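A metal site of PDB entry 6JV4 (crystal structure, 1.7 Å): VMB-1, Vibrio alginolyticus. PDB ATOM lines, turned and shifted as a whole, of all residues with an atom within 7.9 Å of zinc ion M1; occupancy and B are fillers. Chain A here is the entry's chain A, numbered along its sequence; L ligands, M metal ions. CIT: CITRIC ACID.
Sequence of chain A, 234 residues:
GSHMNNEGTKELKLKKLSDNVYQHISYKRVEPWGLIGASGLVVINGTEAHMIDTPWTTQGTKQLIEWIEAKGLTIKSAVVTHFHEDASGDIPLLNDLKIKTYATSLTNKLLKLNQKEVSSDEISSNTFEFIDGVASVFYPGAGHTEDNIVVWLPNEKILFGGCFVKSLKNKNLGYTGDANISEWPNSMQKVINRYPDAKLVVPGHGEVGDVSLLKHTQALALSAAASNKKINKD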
ATOM      1  N   VAL A  30     -12.339  28.047  28.172  1.00  0.00           N
ATOM      2  CA  VAL A  30     -11.931  26.827  28.898  1.00  0.00           C
ATOM      3  C   VAL A  30     -10.507  27.052  29.395  1.00  0.00           C
ATOM      4  O   VAL A  30      -9.602  27.011  28.600  1.00  0.00           O
ATOM      5  CB  VAL A  30     -12.047  25.587  27.987  1.00  0.00           C
ATOM      6  CG1 VAL A  30     -11.719  24.318  28.766  1.00  0.00           C
ATOM      7  CG2 VAL A  30     -13.429  25.456  27.376  1.00  0.00           C
ATOM      8  N   ILE A  36     -12.156  29.120  23.020  1.00  0.00           N
ATOM      9  CA  ILE A  36     -11.987  28.138  21.914  1.00  0.00           C
ATOM     10  C   ILE A  36     -13.337  27.934  21.217  1.00  0.00           C
ATOM     11  O   ILE A  36     -14.383  27.949  21.865  1.00  0.00           O
ATOM     12  CB  ILE A  36     -11.340  26.832  22.393  1.00  0.00           C
ATOM     13  CG1 ILE A  36     -12.180  26.138  23.452  1.00  0.00           C
ATOM     14  CG2 ILE A  36      -9.914  27.093  22.861  1.00  0.00           C
ATOM     15  CD1 ILE A  36     -11.686  24.739  23.840  1.00  0.00           C
ATOM     16  N   GLY A  37     -13.262  27.794  19.894  1.00  0.00           N
ATOM     17  CA  GLY A  37     -14.405  27.586  19.012  1.00  0.00           C
ATOM     18  C   GLY A  37     -14.698  26.086  18.934  1.00  0.00           C
ATOM     19  O   GLY A  37     -13.758  25.304  19.083  1.00  0.00           O
ATOM     20  N   ALA A  38     -15.949  25.713  18.779  1.00  0.00           N
ATOM     21  CA  ALA A  38     -16.345  24.283  18.695  1.00  0.00           C
ATOM     22  C   ALA A  38     -17.250  24.110  17.495  1.00  0.00           C
ATOM     23  O   ALA A  38     -18.173  24.937  17.294  1.00  0.00           O
ATOM     24  CB  ALA A  38     -17.044  23.871  19.934  1.00  0.00           C
ATOM     25  N   SER A  39     -17.054  23.028  16.742  1.00  0.00           N
ATOM     26  CA  SER A  39     -17.861  22.701  15.558  1.00  0.00           C
ATOM     27  C   SER A  39     -18.642  21.397  15.764  1.00  0.00           C
ATOM     28  O   SER A  39     -18.096  20.448  16.282  1.00  0.00           O
ATOM     29  CB  SER A  39     -17.016  22.535  14.341  1.00  0.00           C
ATOM     30  OG  SER A  39     -16.346  23.733  13.996  1.00  0.00           O
ATOM     31  N   ASP A  53     -23.058  16.208  17.140  1.00  0.00           N
ATOM     32  CA  ASP A  53     -22.762  17.031  18.332  1.00  0.00           C
ATOM     33  C   ASP A  53     -23.860  18.097  18.487  1.00  0.00           C
ATOM     34  O   ASP A  53     -24.450  18.553  17.499  1.00  0.00           O
ATOM     35  CB  ASP A  53     -21.344  17.593  18.339  1.00  0.00           C
ATOM     36  CG  ASP A  53     -20.240  16.568  18.576  1.00  0.00           C
ATOM     37  OD1 ASP A  53     -20.557  15.326  18.755  1.00  0.00           O
ATOM     38  OD2 ASP A  53     -19.069  17.032  18.730  1.00  0.00           O
ATOM     39  N   TRP A  56     -22.495  24.125  21.968  1.00  0.00           N
ATOM     40  CA  TRP A  56     -21.899  24.121  23.333  1.00  0.00           C
ATOM     41  C   TRP A  56     -22.777  24.822  24.374  1.00  0.00           C
ATOM     42  O   TRP A  56     -22.582  24.573  25.561  1.00  0.00           O
ATOM     43  CB  TRP A  56     -20.513  24.723  23.228  1.00  0.00           C
ATOM     44  CG  TRP A  56     -19.529  24.232  24.223  1.00  0.00           C
ATOM     45  CD1 TRP A  56     -19.713  23.514  25.368  1.00  0.00           C
ATOM     46  CD2 TRP A  56     -18.120  24.468  24.111  1.00  0.00           C
ATOM     47  NE1 TRP A  56     -18.499  23.264  25.956  1.00  0.00           N
ATOM     48  CE2 TRP A  56     -17.519  23.841  25.211  1.00  0.00           C
ATOM     49  CE3 TRP A  56     -17.345  25.144  23.180  1.00  0.00           C
ATOM     50  CZ2 TRP A  56     -16.146  23.865  25.396  1.00  0.00           C
ATOM     51  CZ3 TRP A  56     -15.978  25.180  23.382  1.00  0.00           C
ATOM     52  CH2 TRP A  56     -15.408  24.520  24.459  1.00  0.00           C
ATOM     53  N   HIS A  82     -18.493  12.367  21.711  1.00  0.00           N
ATOM     54  CA  HIS A  82     -17.842  11.919  22.964  1.00  0.00           C
ATOM     55  C   HIS A  82     -18.594  12.485  24.170  1.00  0.00           C
ATOM     56  O   HIS A  82     -19.560  13.187  23.957  1.00  0.00           O
ATOM     57  CB  HIS A  82     -16.355  12.187  23.040  1.00  0.00           C
ATOM     58  CG  HIS A  82     -15.913  13.588  23.224  1.00  0.00           C
ATOM     59  ND1 HIS A  82     -16.023  14.509  22.227  1.00  0.00           N
ATOM     60  CD2 HIS A  82     -15.273  14.195  24.260  1.00  0.00           C
ATOM     61  CE1 HIS A  82     -15.462  15.657  22.634  1.00  0.00           C
ATOM     62  NE2 HIS A  82     -15.051  15.486  23.895  1.00  0.00           N
ATOM     63  N   HIS A  84     -17.901  14.458  26.673  1.00  0.00           N
ATOM     64  CA  HIS A  84     -17.696  15.839  27.181  1.00  0.00           C
ATOM     65  C   HIS A  84     -18.868  16.744  26.757  1.00  0.00           C
ATOM     66  O   HIS A  84     -19.537  16.513  25.735  1.00  0.00           O
ATOM     67  CB  HIS A  84     -16.343  16.416  26.742  1.00  0.00           C
ATOM     68  CG  HIS A  84     -15.151  15.797  27.366  1.00  0.00           C
ATOM     69  ND1 HIS A  84     -13.907  15.914  26.800  1.00  0.00           N
ATOM     70  CD2 HIS A  84     -14.982  15.051  28.475  1.00  0.00           C
ATOM     71  CE1 HIS A  84     -13.012  15.299  27.557  1.00  0.00           C
ATOM     72  NE2 HIS A  84     -13.653  14.760  28.610  1.00  0.00           N
ATOM     73  N   GLU A  85     -19.039  17.890  27.444  1.00  0.00           N
ATOM     74  CA  GLU A  85     -20.154  18.830  27.248  1.00  0.00           C
ATOM     75  C   GLU A  85     -20.112  19.519  25.885  1.00  0.00           C
ATOM     76  O   GLU A  85     -21.180  19.838  25.372  1.00  0.00           O
ATOM     77  CB  GLU A  85     -20.113  19.909  28.351  1.00  0.00           C
ATOM     78  CG  GLU A  85     -21.279  20.857  28.328  1.00  0.00           C
ATOM     79  CD  GLU A  85     -21.047  22.137  29.126  1.00  0.00           C
ATOM     80  OE1 GLU A  85     -20.046  22.187  29.891  1.00  0.00           O
ATOM     81  OE2 GLU A  85     -21.846  23.049  28.977  1.00  0.00           O
ATOM     82  N   ASP A  86     -18.955  19.724  25.268  1.00  0.00           N
ATOM     83  CA  ASP A  86     -18.936  20.352  23.919  1.00  0.00           C
ATOM     84  C   ASP A  86     -19.578  19.446  22.849  1.00  0.00           C
ATOM     85  O   ASP A  86     -19.909  19.934  21.750  1.00  0.00           O
ATOM     86  CB  ASP A  86     -17.534  20.800  23.500  1.00  0.00           C
ATOM     87  CG  ASP A  86     -16.487  19.739  23.448  1.00  0.00           C
ATOM     88  OD1 ASP A  86     -16.658  18.649  24.063  1.00  0.00           O
ATOM     89  OD2 ASP A  86     -15.439  20.016  22.804  1.00  0.00           O
ATOM     90  N   ALA A  87     -19.630  18.130  23.086  1.00  0.00           N
ATOM     91  CA  ALA A  87     -20.205  17.172  22.121  1.00  0.00           C
ATOM     92  C   ALA A  87     -21.610  16.791  22.544  1.00  0.00           C
ATOM     93  O   ALA A  87     -22.432  16.628  21.651  1.00  0.00           O
ATOM     94  CB  ALA A  87     -19.305  15.982  21.976  1.00  0.00           C
ATOM     95  N   HIS A 144      -8.488  11.391  22.284  1.00  0.00           N
ATOM     96  CA  HIS A 144      -8.916  12.530  23.128  1.00  0.00           C
ATOM     97  C   HIS A 144      -9.664  12.004  24.364  1.00  0.00           C
ATOM     98  O   HIS A 144      -9.453  12.554  25.487  1.00  0.00           O
ATOM     99  CB  HIS A 144      -9.757  13.466  22.296  1.00  0.00           C
ATOM    100  CG  HIS A 144     -10.437  14.503  23.113  1.00  0.00           C
ATOM    101  ND1 HIS A 144      -9.736  15.521  23.714  1.00  0.00           N
ATOM    102  CD2 HIS A 144     -11.729  14.644  23.495  1.00  0.00           C
ATOM    103  CE1 HIS A 144     -10.613  16.294  24.347  1.00  0.00           C
ATOM    104  NE2 HIS A 144     -11.807  15.803  24.230  1.00  0.00           N
ATOM    105  N   GLY A 162     -14.349  15.478  15.226  1.00  0.00           N
ATOM    106  CA  GLY A 162     -14.631  15.854  16.607  1.00  0.00           C
ATOM    107  C   GLY A 162     -13.364  16.108  17.375  1.00  0.00           C
ATOM    108  O   GLY A 162     -12.299  16.435  16.760  1.00  0.00           O
ATOM    109  N   CYS A 163     -13.392  15.945  18.687  1.00  0.00           N
ATOM    110  CA  CYS A 163     -12.217  16.328  19.487  1.00  0.00           C
ATOM    111  C   CYS A 163     -11.058  15.344  19.384  1.00  0.00           C
ATOM    112  O   CYS A 163      -9.976  15.664  19.860  1.00  0.00           O
ATOM    113  CB  CYS A 163     -12.626  16.601  20.924  1.00  0.00           C
ATOM    114  SG  CYS A 163     -13.686  18.081  20.930  1.00  0.00           S
ATOM    115  N   PHE A 164     -11.264  14.191  18.731  1.00  0.00           N
ATOM    116  CA  PHE A 164     -10.191  13.267  18.338  1.00  0.00           C
ATOM    117  C   PHE A 164      -9.248  13.900  17.323  1.00  0.00           C
ATOM    118  O   PHE A 164      -8.080  13.361  17.199  1.00  0.00           O
ATOM    119  CB  PHE A 164     -10.868  12.048  17.722  1.00  0.00           C
ATOM    120  CG  PHE A 164      -9.991  10.921  17.285  1.00  0.00           C
ATOM    121  CD1 PHE A 164      -9.378  10.103  18.224  1.00  0.00           C
ATOM    122  CD2 PHE A 164      -9.824  10.638  15.933  1.00  0.00           C
ATOM    123  CE1 PHE A 164      -8.589   9.043  17.833  1.00  0.00           C
ATOM    124  CE2 PHE A 164      -8.976   9.621  15.552  1.00  0.00           C
ATOM    125  CZ  PHE A 164      -8.392   8.791  16.495  1.00  0.00           C
ATOM    126  N   VAL A 165      -9.697  14.902  16.587  1.00  0.00           N
ATOM    127  CA  VAL A 165      -8.836  15.580  15.562  1.00  0.00           C
ATOM    128  C   VAL A 165      -8.592  17.021  15.994  1.00  0.00           C
ATOM    129  O   VAL A 165      -9.552  17.771  16.263  1.00  0.00           O
ATOM    130  CB  VAL A 165      -9.430  15.493  14.147  1.00  0.00           C
ATOM    131  CG1 VAL A 165      -8.568  16.198  13.115  1.00  0.00           C
ATOM    132  CG2 VAL A 165      -9.704  14.040  13.779  1.00  0.00           C
ATOM    133  N   LYS A 166      -7.311  17.408  16.032  1.00  0.00           N
ATOM    134  CA  LYS A 166      -6.926  18.809  16.329  1.00  0.00           C
ATOM    135  C   LYS A 166      -6.843  19.587  15.016  1.00  0.00           C
ATOM    136  O   LYS A 166      -6.667  19.005  13.940  1.00  0.00           O
ATOM    137  CB  LYS A 166      -5.564  18.835  17.047  1.00  0.00           C
ATOM    138  CG  LYS A 166      -5.474  17.967  18.298  1.00  0.00           C
ATOM    139  CD  LYS A 166      -6.544  18.269  19.330  1.00  0.00           C
ATOM    140  CE  LYS A 166      -6.427  19.620  19.999  1.00  0.00           C
ATOM    141  NZ  LYS A 166      -7.414  19.755  21.111  1.00  0.00           N
ATOM    142  N   LEU A 173      -2.287  19.050  22.346  1.00  0.00           N
ATOM    143  CA  LEU A 173      -3.487  18.194  22.284  1.00  0.00           C
ATOM    144  C   LEU A 173      -4.663  18.838  23.011  1.00  0.00           C
ATOM    145  O   LEU A 173      -5.740  18.288  22.948  1.00  0.00           O
ATOM    146  CB  LEU A 173      -3.170  16.832  22.880  1.00  0.00           C
ATOM    147  CG  LEU A 173      -2.175  15.974  22.071  1.00  0.00           C
ATOM    148  CD1 LEU A 173      -1.795  14.776  22.884  1.00  0.00           C
ATOM    149  CD2 LEU A 173      -2.757  15.592  20.704  1.00  0.00           C
ATOM    150  N   TYR A 175      -7.059  19.568  26.104  1.00  0.00           N
ATOM    151  CA  TYR A 175      -7.360  18.944  27.402  1.00  0.00           C
ATOM    152  C   TYR A 175      -7.087  17.443  27.331  1.00  0.00           C
ATOM    153  O   TYR A 175      -7.749  16.719  26.538  1.00  0.00           O
ATOM    154  CB  TYR A 175      -8.803  19.173  27.815  1.00  0.00           C
ATOM    155  CG  TYR A 175      -9.143  18.466  29.091  1.00  0.00           C
ATOM    156  CD1 TYR A 175      -8.526  18.824  30.269  1.00  0.00           C
ATOM    157  CD2 TYR A 175     -10.037  17.403  29.118  1.00  0.00           C
ATOM    158  CE1 TYR A 175      -8.868  18.205  31.453  1.00  0.00           C
ATOM    159  CE2 TYR A 175     -10.380  16.765  30.286  1.00  0.00           C
ATOM    160  CZ  TYR A 175      -9.809  17.178  31.471  1.00  0.00           C
ATOM    161  OH  TYR A 175     -10.095  16.537  32.639  1.00  0.00           O
ATOM    162  N   PRO A 203     -12.327  19.390  12.606  1.00  0.00           N
ATOM    163  CA  PRO A 203     -11.892  19.169  13.971  1.00  0.00           C
ATOM    164  C   PRO A 203     -12.949  19.687  14.932  1.00  0.00           C
ATOM    165  O   PRO A 203     -13.771  20.518  14.586  1.00  0.00           O
ATOM    166  CB  PRO A 203     -10.591  19.916  14.059  1.00  0.00           C
ATOM    167  CG  PRO A 203     -10.884  21.160  13.213  1.00  0.00           C
ATOM    168  CD  PRO A 203     -11.724  20.635  12.076  1.00  0.00           C
ATOM    169  N   GLY A 204     -12.911  19.150  16.157  1.00  0.00           N
ATOM    170  CA  GLY A 204     -13.825  19.589  17.218  1.00  0.00           C
ATOM    171  C   GLY A 204     -13.663  21.055  17.552  1.00  0.00           C
ATOM    172  O   GLY A 204     -14.672  21.704  17.937  1.00  0.00           O
ATOM    173  N   HIS A 205     -12.438  21.561  17.490  1.00  0.00           N
ATOM    174  CA  HIS A 205     -12.101  22.985  17.720  1.00  0.00           C
ATOM    175  C   HIS A 205     -11.255  23.499  16.580  1.00  0.00           C
ATOM    176  O   HIS A 205     -10.435  22.738  16.047  1.00  0.00           O
ATOM    177  CB  HIS A 205     -11.352  23.184  19.058  1.00  0.00           C
ATOM    178  CG  HIS A 205     -12.062  22.559  20.193  1.00  0.00           C
ATOM    179  ND1 HIS A 205     -13.250  23.050  20.667  1.00  0.00           N
ATOM    180  CD2 HIS A 205     -11.831  21.452  20.924  1.00  0.00           C
ATOM    181  CE1 HIS A 205     -13.733  22.273  21.611  1.00  0.00           C
ATOM    182  NE2 HIS A 205     -12.903  21.297  21.775  1.00  0.00           N
HETATM  183  C1  CIT L   1     -14.029  20.829  27.507  1.00  0.00           C
HETATM  184  O1  CIT L   1     -14.182  21.208  28.682  1.00  0.00           O
HETATM  185  O2  CIT L   1     -14.945  20.400  26.790  1.00  0.00           O
HETATM  186  C2  CIT L   1     -12.630  20.915  26.907  1.00  0.00           C
HETATM  187  C3  CIT L   1     -12.508  20.444  25.456  1.00  0.00           C
HETATM  188  O7  CIT L   1     -13.486  21.084  24.662  1.00  0.00           O
HETATM  189  C4  CIT L   1     -11.110  20.810  24.934  1.00  0.00           C
HETATM  190  C5  CIT L   1     -10.548  19.880  23.866  1.00  0.00           C
HETATM  191  O3  CIT L   1      -9.319  19.696  23.843  1.00  0.00           O
HETATM  192  O4  CIT L   1     -11.342  19.341  23.081  1.00  0.00           O
HETATM  193  C6  CIT L   1     -12.697  18.906  25.396  1.00  0.00           C
HETATM  194  O5  CIT L   1     -12.120  18.218  26.264  1.00  0.00           O
HETATM  195  O6  CIT L   1     -13.408  18.454  24.477  1.00  0.00           O
HETATM  196 ZN    ZN M   1     -13.434  19.510  22.771  1.00  0.00          ZN
HETATM  197 ZN    ZN M   2     -13.550  16.572  24.950  1.00  0.00          ZN
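ND1 of His 205 is in hydrogen-bond range of O of Gly 37, 2.8 Å away.
Within 4 Å of zinc ion M1: Asp 86, Cys 163 and His 205. The nearest printed residue that does not touch zinc ion M1 is His 144 (4.3 Å).
Zinc ion M1 is bound by O6 of the ligand (2.0 Å), OD2 of Asp 86 (2.1 Å), NE2 of His 205 (2.1 Å), O4 of the ligand (2.1 Å), SG of Cys 163 (2.3 Å) and O7 of the ligand (2.5 Å).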
